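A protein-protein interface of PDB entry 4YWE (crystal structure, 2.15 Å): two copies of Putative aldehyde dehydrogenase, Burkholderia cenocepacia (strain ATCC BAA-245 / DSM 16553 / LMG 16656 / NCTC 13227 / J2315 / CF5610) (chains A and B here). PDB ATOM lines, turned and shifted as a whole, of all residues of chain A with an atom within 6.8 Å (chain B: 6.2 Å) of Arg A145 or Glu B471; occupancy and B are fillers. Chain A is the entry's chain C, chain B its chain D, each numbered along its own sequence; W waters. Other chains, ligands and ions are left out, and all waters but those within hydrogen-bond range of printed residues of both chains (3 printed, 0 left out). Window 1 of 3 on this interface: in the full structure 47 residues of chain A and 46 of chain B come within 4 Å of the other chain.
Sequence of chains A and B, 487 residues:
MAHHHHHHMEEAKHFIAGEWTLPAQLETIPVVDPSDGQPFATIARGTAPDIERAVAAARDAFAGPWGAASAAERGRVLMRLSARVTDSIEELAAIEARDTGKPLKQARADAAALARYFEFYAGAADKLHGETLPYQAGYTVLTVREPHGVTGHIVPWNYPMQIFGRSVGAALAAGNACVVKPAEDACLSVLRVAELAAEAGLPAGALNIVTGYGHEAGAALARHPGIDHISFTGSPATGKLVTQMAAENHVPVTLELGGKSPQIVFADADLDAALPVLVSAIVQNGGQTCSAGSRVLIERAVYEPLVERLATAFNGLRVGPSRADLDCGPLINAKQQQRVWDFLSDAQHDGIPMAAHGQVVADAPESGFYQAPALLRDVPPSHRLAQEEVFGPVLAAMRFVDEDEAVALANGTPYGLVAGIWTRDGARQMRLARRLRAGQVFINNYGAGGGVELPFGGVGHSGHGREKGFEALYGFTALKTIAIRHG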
ATOM      1  N   LEU A 128      10.659 -25.946  20.813  1.00  0.00           N
ATOM      2  CA  LEU A 128       9.519 -25.547  21.628  1.00  0.00           C
ATOM      3  C   LEU A 128       8.532 -26.703  21.682  1.00  0.00           C
ATOM      4  O   LEU A 128       7.757 -26.916  20.750  1.00  0.00           O
ATOM      5  CB  LEU A 128       8.851 -24.288  21.071  1.00  0.00           C
ATOM      6  CG  LEU A 128       7.613 -23.796  21.824  1.00  0.00           C
ATOM      7  CD1 LEU A 128       7.924 -23.594  23.300  1.00  0.00           C
ATOM      8  CD2 LEU A 128       7.087 -22.508  21.206  1.00  0.00           C
ATOM      9  N   HIS A 129       8.568 -27.452  22.776  1.00  0.00           N
ATOM     10  CA  HIS A 129       7.797 -28.683  22.881  1.00  0.00           C
ATOM     11  C   HIS A 129       6.432 -28.480  23.523  1.00  0.00           C
ATOM     12  O   HIS A 129       6.261 -27.633  24.400  1.00  0.00           O
ATOM     13  CB  HIS A 129       8.579 -29.728  23.682  1.00  0.00           C
ATOM     14  CG  HIS A 129       9.904 -30.079  23.082  1.00  0.00           C
ATOM     15  ND1 HIS A 129      10.905 -30.698  23.800  1.00  0.00           N
ATOM     16  CD2 HIS A 129      10.394 -29.900  21.832  1.00  0.00           C
ATOM     17  CE1 HIS A 129      11.955 -30.885  23.019  1.00  0.00           C
ATOM     18  NE2 HIS A 129      11.669 -30.411  21.820  1.00  0.00           N
ATOM     19  N   GLY A 130       5.464 -29.269  23.073  1.00  0.00           N
ATOM     20  CA  GLY A 130       4.206 -29.405  23.776  1.00  0.00           C
ATOM     21  C   GLY A 130       4.314 -30.593  24.711  1.00  0.00           C
ATOM     22  O   GLY A 130       5.420 -31.007  25.059  1.00  0.00           O
ATOM     23  N   GLU A 131       3.181 -31.156  25.111  1.00  0.00           N
ATOM     24  CA  GLU A 131       3.196 -32.264  26.061  1.00  0.00           C
ATOM     25  C   GLU A 131       2.178 -33.345  25.728  1.00  0.00           C
ATOM     26  O   GLU A 131       1.271 -33.141  24.922  1.00  0.00           O
ATOM     27  CB  GLU A 131       2.932 -31.752  27.476  1.00  0.00           C
ATOM     28  CG  GLU A 131       4.053 -30.919  28.064  1.00  0.00           C
ATOM     29  CD  GLU A 131       3.692 -30.341  29.415  1.00  0.00           C
ATOM     30  OE1 GLU A 131       2.721 -29.558  29.484  1.00  0.00           O
ATOM     31  OE2 GLU A 131       4.374 -30.675  30.407  1.00  0.00           O
ATOM     32  N   THR A 143      -0.696 -31.907  23.813  1.00  0.00           N
ATOM     33  CA  THR A 143      -0.817 -30.456  23.774  1.00  0.00           C
ATOM     34  C   THR A 143       0.138 -29.885  22.738  1.00  0.00           C
ATOM     35  O   THR A 143       1.287 -30.312  22.641  1.00  0.00           O
ATOM     36  CB  THR A 143      -0.527 -29.816  25.145  1.00  0.00           C
ATOM     37  OG1 THR A 143       0.866 -29.947  25.457  1.00  0.00           O
ATOM     38  CG2 THR A 143      -1.361 -30.480  26.232  1.00  0.00           C
ATOM     39  N   VAL A 144      -0.347 -28.924  21.961  1.00  0.00           N
ATOM     40  CA  VAL A 144       0.459 -28.302  20.921  1.00  0.00           C
ATOM     41  C   VAL A 144       0.517 -26.797  21.141  1.00  0.00           C
ATOM     42  O   VAL A 144      -0.517 -26.144  21.282  1.00  0.00           O
ATOM     43  CB  VAL A 144      -0.089 -28.629  19.520  1.00  0.00           C
ATOM     44  CG1 VAL A 144       0.697 -27.882  18.455  1.00  0.00           C
ATOM     45  CG2 VAL A 144      -0.050 -30.131  19.268  1.00  0.00           C
ATOM     46  N   ARG A 145       1.728 -26.253  21.175  1.00  0.00           N
ATOM     47  CA  ARG A 145       1.914 -24.817  21.347  1.00  0.00           C
ATOM     48  C   ARG A 145       1.940 -24.127  19.990  1.00  0.00           C
ATOM     49  O   ARG A 145       2.936 -24.179  19.269  1.00  0.00           O
ATOM     50  CB  ARG A 145       3.196 -24.528  22.127  1.00  0.00           C
ATOM     51  CG  ARG A 145       3.224 -25.179  23.501  1.00  0.00           C
ATOM     52  CD  ARG A 145       4.402 -24.705  24.334  1.00  0.00           C
ATOM     53  NE  ARG A 145       4.456 -25.388  25.624  1.00  0.00           N
ATOM     54  CZ  ARG A 145       3.744 -25.034  26.690  1.00  0.00           C
ATOM     55  NH1 ARG A 145       2.915 -23.999  26.625  1.00  0.00           N
ATOM     56  NH2 ARG A 145       3.859 -25.715  27.821  1.00  0.00           N
ATOM     57  N   GLU A 146       0.829 -23.483  19.648  1.00  0.00           N
ATOM     58  CA  GLU A 146       0.677 -22.841  18.350  1.00  0.00           C
ATOM     59  C   GLU A 146       0.895 -21.338  18.448  1.00  0.00           C
ATOM     60  O   GLU A 146       0.519 -20.720  19.443  1.00  0.00           O
ATOM     61  CB  GLU A 146      -0.713 -23.124  17.773  1.00  0.00           C
ATOM     62  CG  GLU A 146      -0.996 -24.590  17.501  1.00  0.00           C
ATOM     63  CD  GLU A 146      -2.466 -24.855  17.248  1.00  0.00           C
ATOM     64  OE1 GLU A 146      -3.296 -24.000  17.624  1.00  0.00           O
ATOM     65  OE2 GLU A 146      -2.793 -25.912  16.669  1.00  0.00           O
ATOM     66  N   PRO A 147       1.497 -20.743  17.408  1.00  0.00           N
ATOM     67  CA  PRO A 147       1.636 -19.285  17.347  1.00  0.00           C
ATOM     68  C   PRO A 147       0.282 -18.591  17.407  1.00  0.00           C
ATOM     69  O   PRO A 147      -0.725 -19.185  17.012  1.00  0.00           O
ATOM     70  CB  PRO A 147       2.314 -19.049  15.991  1.00  0.00           C
ATOM     71  CG  PRO A 147       2.022 -20.282  15.197  1.00  0.00           C
ATOM     72  CD  PRO A 147       2.014 -21.397  16.194  1.00  0.00           C
ATOM     73  N   ALA A 174       8.522 -18.380  17.228  1.00  0.00           N
ATOM     74  CA  ALA A 174       7.296 -19.039  17.661  1.00  0.00           C
ATOM     75  C   ALA A 174       6.385 -19.362  16.478  1.00  0.00           C
ATOM     76  O   ALA A 174       5.495 -20.206  16.584  1.00  0.00           O
ATOM     77  CB  ALA A 174       6.564 -18.176  18.674  1.00  0.00           C
ATOM     78  N   LEU A 473       8.933 -17.624  24.434  1.00  0.00           N
ATOM     79  CA  LEU A 473       8.224 -18.398  23.419  1.00  0.00           C
ATOM     80  C   LEU A 473       6.819 -18.791  23.870  1.00  0.00           C
ATOM     81  O   LEU A 473       5.918 -18.946  23.046  1.00  0.00           O
ATOM     82  CB  LEU A 473       9.020 -19.653  23.054  1.00  0.00           C
ATOM     83  CG  LEU A 473      10.392 -19.418  22.425  1.00  0.00           C
ATOM     84  CD1 LEU A 473      11.139 -20.733  22.265  1.00  0.00           C
ATOM     85  CD2 LEU A 473      10.250 -18.711  21.086  1.00  0.00           C
ATOM     86  N   TYR A 474       6.635 -18.957  25.176  1.00  0.00           N
ATOM     87  CA  TYR A 474       5.330 -19.326  25.711  1.00  0.00           C
ATOM     88  C   TYR A 474       4.369 -18.146  25.634  1.00  0.00           C
ATOM     89  O   TYR A 474       3.157 -18.326  25.516  1.00  0.00           O
ATOM     90  CB  TYR A 474       5.454 -19.818  27.153  1.00  0.00           C
ATOM     91  CG  TYR A 474       6.382 -21.000  27.318  1.00  0.00           C
ATOM     92  CD1 TYR A 474       6.011 -22.264  26.880  1.00  0.00           C
ATOM     93  CD2 TYR A 474       7.625 -20.853  27.919  1.00  0.00           C
ATOM     94  CE1 TYR A 474       6.856 -23.349  27.030  1.00  0.00           C
ATOM     95  CE2 TYR A 474       8.477 -21.932  28.075  1.00  0.00           C
ATOM     96  CZ  TYR A 474       8.087 -23.178  27.629  1.00  0.00           C
ATOM     97  OH  TYR A 474       8.931 -24.254  27.781  1.00  0.00           O
ATOM     98  N   THR A 477       3.009 -17.929  22.036  1.00  0.00           N
ATOM     99  CA  THR A 477       2.247 -19.086  21.584  1.00  0.00           C
ATOM    100  C   THR A 477       1.020 -19.295  22.463  1.00  0.00           C
ATOM    101  O   THR A 477       0.926 -18.745  23.560  1.00  0.00           O
ATOM    102  CB  THR A 477       3.092 -20.376  21.586  1.00  0.00           C
ATOM    103  OG1 THR A 477       3.751 -20.520  22.850  1.00  0.00           O
ATOM    104  CG2 THR A 477       4.133 -20.339  20.476  1.00  0.00           C
ATOM    105  N   ALA A 478       0.075 -20.083  21.963  1.00  0.00           N
ATOM    106  CA  ALA A 478      -1.122 -20.430  22.716  1.00  0.00           C
ATOM    107  C   ALA A 478      -1.289 -21.943  22.719  1.00  0.00           C
ATOM    108  O   ALA A 478      -1.042 -22.605  21.711  1.00  0.00           O
ATOM    109  CB  ALA A 478      -2.348 -19.750  22.128  1.00  0.00           C
ATOM    110  N   LEU A 479      -1.705 -22.489  23.855  1.00  0.00           N
ATOM    111  CA  LEU A 479      -1.766 -23.933  24.023  1.00  0.00           C
ATOM    112  C   LEU A 479      -3.080 -24.521  23.518  1.00  0.00           C
ATOM    113  O   LEU A 479      -4.161 -24.124  23.954  1.00  0.00           O
ATOM    114  CB  LEU A 479      -1.570 -24.304  25.495  1.00  0.00           C
ATOM    115  CG  LEU A 479      -1.274 -25.780  25.767  1.00  0.00           C
ATOM    116  CD1 LEU A 479       0.121 -26.131  25.276  1.00  0.00           C
ATOM    117  CD2 LEU A 479      -1.429 -26.101  27.244  1.00  0.00           C
ATOM    118  N   LYS A 480      -2.975 -25.469  22.592  1.00  0.00           N
ATOM    119  CA  LYS A 480      -4.125 -26.250  22.162  1.00  0.00           C
ATOM    120  C   LYS A 480      -3.989 -27.668  22.699  1.00  0.00           C
ATOM    121  O   LYS A 480      -2.917 -28.267  22.619  1.00  0.00           O
ATOM    122  CB  LYS A 480      -4.246 -26.270  20.636  1.00  0.00           C
ATOM    123  CG  LYS A 480      -5.227 -27.316  20.114  1.00  0.00           C
ATOM    124  CD  LYS A 480      -5.165 -27.451  18.603  1.00  0.00           C
ATOM    125  CE  LYS A 480      -5.718 -26.215  17.915  1.00  0.00           C
ATOM    126  NZ  LYS A 480      -5.443 -26.228  16.451  1.00  0.00           N
ATOM    127  N   TYR B 121      -4.604 -30.821  42.119  1.00  0.00           N
ATOM    128  CA  TYR B 121      -3.698 -29.725  42.442  1.00  0.00           C
ATOM    129  C   TYR B 121      -2.990 -29.930  43.780  1.00  0.00           C
ATOM    130  O   TYR B 121      -1.968 -29.299  44.049  1.00  0.00           O
ATOM    131  CB  TYR B 121      -4.459 -28.399  42.434  1.00  0.00           C
ATOM    132  CG  TYR B 121      -4.752 -27.909  41.036  1.00  0.00           C
ATOM    133  CD1 TYR B 121      -3.738 -27.820  40.091  1.00  0.00           C
ATOM    134  CD2 TYR B 121      -6.039 -27.560  40.653  1.00  0.00           C
ATOM    135  CE1 TYR B 121      -3.994 -27.384  38.809  1.00  0.00           C
ATOM    136  CE2 TYR B 121      -6.305 -27.120  39.370  1.00  0.00           C
ATOM    137  CZ  TYR B 121      -5.277 -27.035  38.452  1.00  0.00           C
ATOM    138  OH  TYR B 121      -5.531 -26.602  37.173  1.00  0.00           O
ATOM    139  N   ARG B 434      -5.317 -29.591  13.935  1.00  0.00           N
ATOM    140  CA  ARG B 434      -4.315 -28.541  13.798  1.00  0.00           C
ATOM    141  C   ARG B 434      -4.909 -27.288  13.151  1.00  0.00           C
ATOM    142  O   ARG B 434      -4.491 -26.171  13.452  1.00  0.00           O
ATOM    143  CB  ARG B 434      -3.120 -29.039  12.980  1.00  0.00           C
ATOM    144  CG  ARG B 434      -2.503 -30.331  13.498  1.00  0.00           C
ATOM    145  CD  ARG B 434      -2.002 -30.194  14.927  1.00  0.00           C
ATOM    146  NE  ARG B 434      -0.597 -29.796  14.985  1.00  0.00           N
ATOM    147  CZ  ARG B 434      -0.176 -28.541  15.093  1.00  0.00           C
ATOM    148  NH1 ARG B 434       1.123 -28.278  15.138  1.00  0.00           N
ATOM    149  NH2 ARG B 434      -1.052 -27.547  15.161  1.00  0.00           N
ATOM    150  N   PRO B 455      -5.959 -28.633  30.013  1.00  0.00           N
ATOM    151  CA  PRO B 455      -5.870 -27.173  29.918  1.00  0.00           C
ATOM    152  C   PRO B 455      -7.003 -26.593  29.080  1.00  0.00           C
ATOM    153  O   PRO B 455      -7.236 -27.039  27.956  1.00  0.00           O
ATOM    154  CB  PRO B 455      -4.513 -26.949  29.248  1.00  0.00           C
ATOM    155  CG  PRO B 455      -3.713 -28.145  29.637  1.00  0.00           C
ATOM    156  CD  PRO B 455      -4.691 -29.285  29.645  1.00  0.00           C
ATOM    157  N   ARG B 466      -5.018 -19.902  29.939  1.00  0.00           N
ATOM    158  CA  ARG B 466      -5.442 -21.276  30.172  1.00  0.00           C
ATOM    159  C   ARG B 466      -5.615 -21.578  31.656  1.00  0.00           C
ATOM    160  O   ARG B 466      -4.789 -21.190  32.480  1.00  0.00           O
ATOM    161  CB  ARG B 466      -4.434 -22.255  29.564  1.00  0.00           C
ATOM    162  CG  ARG B 466      -4.305 -22.169  28.054  1.00  0.00           C
ATOM    163  CD  ARG B 466      -5.589 -22.602  27.363  1.00  0.00           C
ATOM    164  NE  ARG B 466      -5.470 -22.538  25.910  1.00  0.00           N
ATOM    165  CZ  ARG B 466      -5.873 -21.510  25.170  1.00  0.00           C
ATOM    166  NH1 ARG B 466      -6.431 -20.453  25.746  1.00  0.00           N
ATOM    167  NH2 ARG B 466      -5.723 -21.541  23.853  1.00  0.00           N
ATOM    168  N   GLU B 467      -6.703 -22.265  31.987  1.00  0.00           N
ATOM    169  CA  GLU B 467      -6.880 -22.835  33.315  1.00  0.00           C
ATOM    170  C   GLU B 467      -7.251 -24.309  33.163  1.00  0.00           C
ATOM    171  O   GLU B 467      -7.356 -24.801  32.039  1.00  0.00           O
ATOM    172  CB  GLU B 467      -7.928 -22.058  34.114  1.00  0.00           C
ATOM    173  CG  GLU B 467      -7.446 -20.664  34.507  1.00  0.00           C
ATOM    174  CD  GLU B 467      -8.389 -19.943  35.448  1.00  0.00           C
ATOM    175  OE1 GLU B 467      -9.356 -20.570  35.929  1.00  0.00           O
ATOM    176  OE2 GLU B 467      -8.157 -18.743  35.709  1.00  0.00           O
ATOM    177  N   LYS B 468      -7.434 -24.996  34.291  1.00  0.00           N
ATOM    178  CA  LYS B 468      -7.470 -26.464  34.365  1.00  0.00           C
ATOM    179  C   LYS B 468      -6.100 -27.056  34.039  1.00  0.00           C
ATOM    180  O   LYS B 468      -5.248 -26.395  33.443  1.00  0.00           O
ATOM    181  CB  LYS B 468      -8.522 -27.074  33.428  1.00  0.00           C
ATOM    182  CG  LYS B 468      -9.956 -26.685  33.705  1.00  0.00           C
ATOM    183  CD  LYS B 468     -10.900 -27.457  32.793  1.00  0.00           C
ATOM    184  CE  LYS B 468     -12.287 -26.836  32.761  1.00  0.00           C
ATOM    185  NZ  LYS B 468     -13.190 -27.548  31.811  1.00  0.00           N
ATOM    186  N   GLY B 469      -5.896 -28.308  34.435  1.00  0.00           N
ATOM    187  CA  GLY B 469      -4.651 -29.004  34.165  1.00  0.00           C
ATOM    188  C   GLY B 469      -3.449 -28.424  34.884  1.00  0.00           C
ATOM    189  O   GLY B 469      -3.575 -27.487  35.672  1.00  0.00           O
ATOM    190  N   PHE B 470      -2.276 -28.983  34.608  1.00  0.00           N
ATOM    191  CA  PHE B 470      -1.040 -28.508  35.221  1.00  0.00           C
ATOM    192  C   PHE B 470      -0.682 -27.120  34.697  1.00  0.00           C
ATOM    193  O   PHE B 470      -0.102 -26.306  35.416  1.00  0.00           O
ATOM    194  CB  PHE B 470       0.102 -29.490  34.951  1.00  0.00           C
ATOM    195  CG  PHE B 470       1.267 -29.340  35.889  1.00  0.00           C
ATOM    196  CD1 PHE B 470       1.275 -29.996  37.111  1.00  0.00           C
ATOM    197  CD2 PHE B 470       2.352 -28.549  35.552  1.00  0.00           C
ATOM    198  CE1 PHE B 470       2.344 -29.864  37.979  1.00  0.00           C
ATOM    199  CE2 PHE B 470       3.426 -28.413  36.416  1.00  0.00           C
ATOM    200  CZ  PHE B 470       3.420 -29.071  37.632  1.00  0.00           C
ATOM    201  N   GLU B 471      -1.048 -26.863  33.443  1.00  0.00           N
ATOM    202  CA  GLU B 471      -0.753 -25.603  32.764  1.00  0.00           C
ATOM    203  C   GLU B 471      -1.262 -24.387  33.539  1.00  0.00           C
ATOM    204  O   GLU B 471      -0.692 -23.300  33.452  1.00  0.00           O
ATOM    205  CB  GLU B 471      -1.363 -25.614  31.358  1.00  0.00           C
ATOM    206  CG  GLU B 471      -0.966 -24.437  30.481  1.00  0.00           C
ATOM    207  CD  GLU B 471       0.421 -24.593  29.884  1.00  0.00           C
ATOM    208  OE1 GLU B 471       1.011 -25.686  30.019  1.00  0.00           O
ATOM    209  OE2 GLU B 471       0.920 -23.623  29.277  1.00  0.00           O
ATOM    210  N   ALA B 472      -2.334 -24.586  34.300  1.00  0.00           N
ATOM    211  CA  ALA B 472      -2.971 -23.507  35.051  1.00  0.00           C
ATOM    212  C   ALA B 472      -2.032 -22.858  36.066  1.00  0.00           C
ATOM    213  O   ALA B 472      -2.146 -21.665  36.344  1.00  0.00           O
ATOM    214  CB  ALA B 472      -4.212 -24.027  35.753  1.00  0.00           C
ATOM    215  N   LEU B 473      -1.108 -23.641  36.614  1.00  0.00           N
ATOM    216  CA  LEU B 473      -0.186 -23.140  37.630  1.00  0.00           C
ATOM    217  C   LEU B 473       0.742 -22.051  37.089  1.00  0.00           C
ATOM    218  O   LEU B 473       1.231 -21.212  37.848  1.00  0.00           O
ATOM    219  CB  LEU B 473       0.646 -24.287  38.208  1.00  0.00           C
ATOM    220  CG  LEU B 473      -0.126 -25.376  38.955  1.00  0.00           C
ATOM    221  CD1 LEU B 473       0.797 -26.527  39.316  1.00  0.00           C
ATOM    222  CD2 LEU B 473      -0.794 -24.806  40.202  1.00  0.00           C
ATOM    223  N   TYR B 474       0.983 -22.065  35.782  1.00  0.00           N
ATOM    224  CA  TYR B 474       1.841 -21.062  35.158  1.00  0.00           C
ATOM    225  C   TYR B 474       1.127 -19.718  35.071  1.00  0.00           C
ATOM    226  O   TYR B 474       1.761 -18.662  35.081  1.00  0.00           O
ATOM    227  CB  TYR B 474       2.281 -21.513  33.764  1.00  0.00           C
ATOM    228  CG  TYR B 474       3.051 -22.814  33.747  1.00  0.00           C
ATOM    229  CD1 TYR B 474       4.373 -22.869  34.170  1.00  0.00           C
ATOM    230  CD2 TYR B 474       2.458 -23.987  33.297  1.00  0.00           C
ATOM    231  CE1 TYR B 474       5.080 -24.057  34.152  1.00  0.00           C
ATOM    232  CE2 TYR B 474       3.157 -25.179  33.275  1.00  0.00           C
ATOM    233  CZ  TYR B 474       4.467 -25.209  33.704  1.00  0.00           C
ATOM    234  OH  TYR B 474       5.165 -26.395  33.683  1.00  0.00           O
ATOM    235  N   GLY B 475      -0.198 -19.765  34.980  1.00  0.00           N
ATOM    236  CA  GLY B 475      -0.999 -18.559  34.917  1.00  0.00           C
ATOM    237  C   GLY B 475      -1.185 -17.913  36.276  1.00  0.00           C
ATOM    238  O   GLY B 475      -1.534 -16.736  36.372  1.00  0.00           O
ATOM    239  N   PHE B 476      -0.951 -18.690  37.330  1.00  0.00           N
ATOM    240  CA  PHE B 476      -1.101 -18.195  38.694  1.00  0.00           C
ATOM    241  C   PHE B 476       0.251 -17.986  39.374  1.00  0.00           C
ATOM    242  O   PHE B 476       0.321 -17.799  40.588  1.00  0.00           O
ATOM    243  CB  PHE B 476      -1.960 -19.156  39.523  1.00  0.00           C
ATOM    244  CG  PHE B 476      -3.419 -19.129  39.166  1.00  0.00           C
ATOM    245  CD1 PHE B 476      -4.228 -18.081  39.579  1.00  0.00           C
ATOM    246  CD2 PHE B 476      -3.986 -20.154  38.427  1.00  0.00           C
ATOM    247  CE1 PHE B 476      -5.574 -18.053  39.255  1.00  0.00           C
ATOM    248  CE2 PHE B 476      -5.335 -20.134  38.102  1.00  0.00           C
ATOM    249  CZ  PHE B 476      -6.127 -19.082  38.516  1.00  0.00           C
HETATM  250  O   HOH W   1       3.982 -28.722  32.643  1.00  0.00           O
HETATM  251  O   HOH W   2      -5.550 -25.860  26.078  1.00  0.00           O
HETATM  252  O   HOH W   3       1.218 -28.068  31.062  1.00  0.00           O
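NH1 of Arg A145 is in salt-bridge range of OE2 of Glu B471, 3.3 Å away.
The side-chain carboxylate of Glu A146 is in salt-bridge range of the guanidinium group of Arg B434.
O of Leu A479 lies within hydrogen-bond range of NE of Arg B466 (2.8 Å).
The backbone carbonyl oxygen (O) of Arg B434 lies within hydrogen-bond range of the side-chain amino group (NZ) of Lys A480 (3.1 Å).
The backbone carbonyl oxygen (O) of His A129 lies within hydrogen-bond range of the guanidinium group (NE) of Arg A145 (3.1 Å).
The backbone carbonyl oxygen of Lys A480 lies within hydrogen-bond range of the backbone NH of Val A144, 2.7 Å away.
The backbone NH (N) of Ala A478 lies within hydrogen-bond range of the backbone carbonyl oxygen (O) of Glu A146 (2.6 Å).
NZ of Lys A480 is in salt-bridge range of OE2 of Glu A146, 2.7 Å away.
Among the printed residues, merely in contact across the chains: Val A144 with Arg B434 (3.4 Å), Leu A479 with Glu B471 (3.6 Å) and Leu A479 with Pro B455 (3.8 Å).
Arg A145 touches just one residue of chain B: Glu B471 (3.3 Å).
Glu B471 touches two residues of chain A.
Of the printed residues of chain A, Arg B466 touches Leu A479.
Printed residues of chain B within 4 Å of Leu A479: Pro B455 (3.8 Å), Arg B466 (2.8 Å) and Glu B471 (3.6 Å).
Printed residues of chain B within 4 Å of Glu A146: Arg B434 (2.8 Å).
Lys B468 touches none of the printed residues of chain A.
The nearest residue of chain A that does not touch Glu B471 is Glu A131 (4.3 Å).
The nearest printed residue of chain B that does not touch Leu A479 is Ala B472 (7.3 Å).
Of the 16 printed residues of chain A, 5 touch a printed residue of chain B.
Printed residues of chain A that touch a printed residue of chain B: Val A144, Arg A145, Glu A146, Leu A479 and Lys A480.
Hydrophobic or aromatic side chains of chain A within 4 Å of the printed part of chain B: Val A144 and Leu A479.
Along chain A the printed residues that touch a printed residue of chain B span positions 144 to 480.
Hydrophobic or aromatic side chains of chain B that line the printed part of chain A: Pro B455.
Positions printed for both chains: 473 and 474.
Of the 7 pairs that touch across the chains among the printed residues, none has its exchanged pair printed and touching as well.
Water W3 lies within hydrogen-bond range of OE1 of Glu B471 and OE1 of Glu A131.
Water W2 lies within hydrogen-bond range of O of Pro B455 (2.8 Å), O of Leu A479 (3.1 Å) and NE of Arg B466 (3.3 Å).
Water W1 lies within hydrogen-bond range of OH of Tyr B474 (2.8 Å) and OE2 of Glu A131 (3.0 Å).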
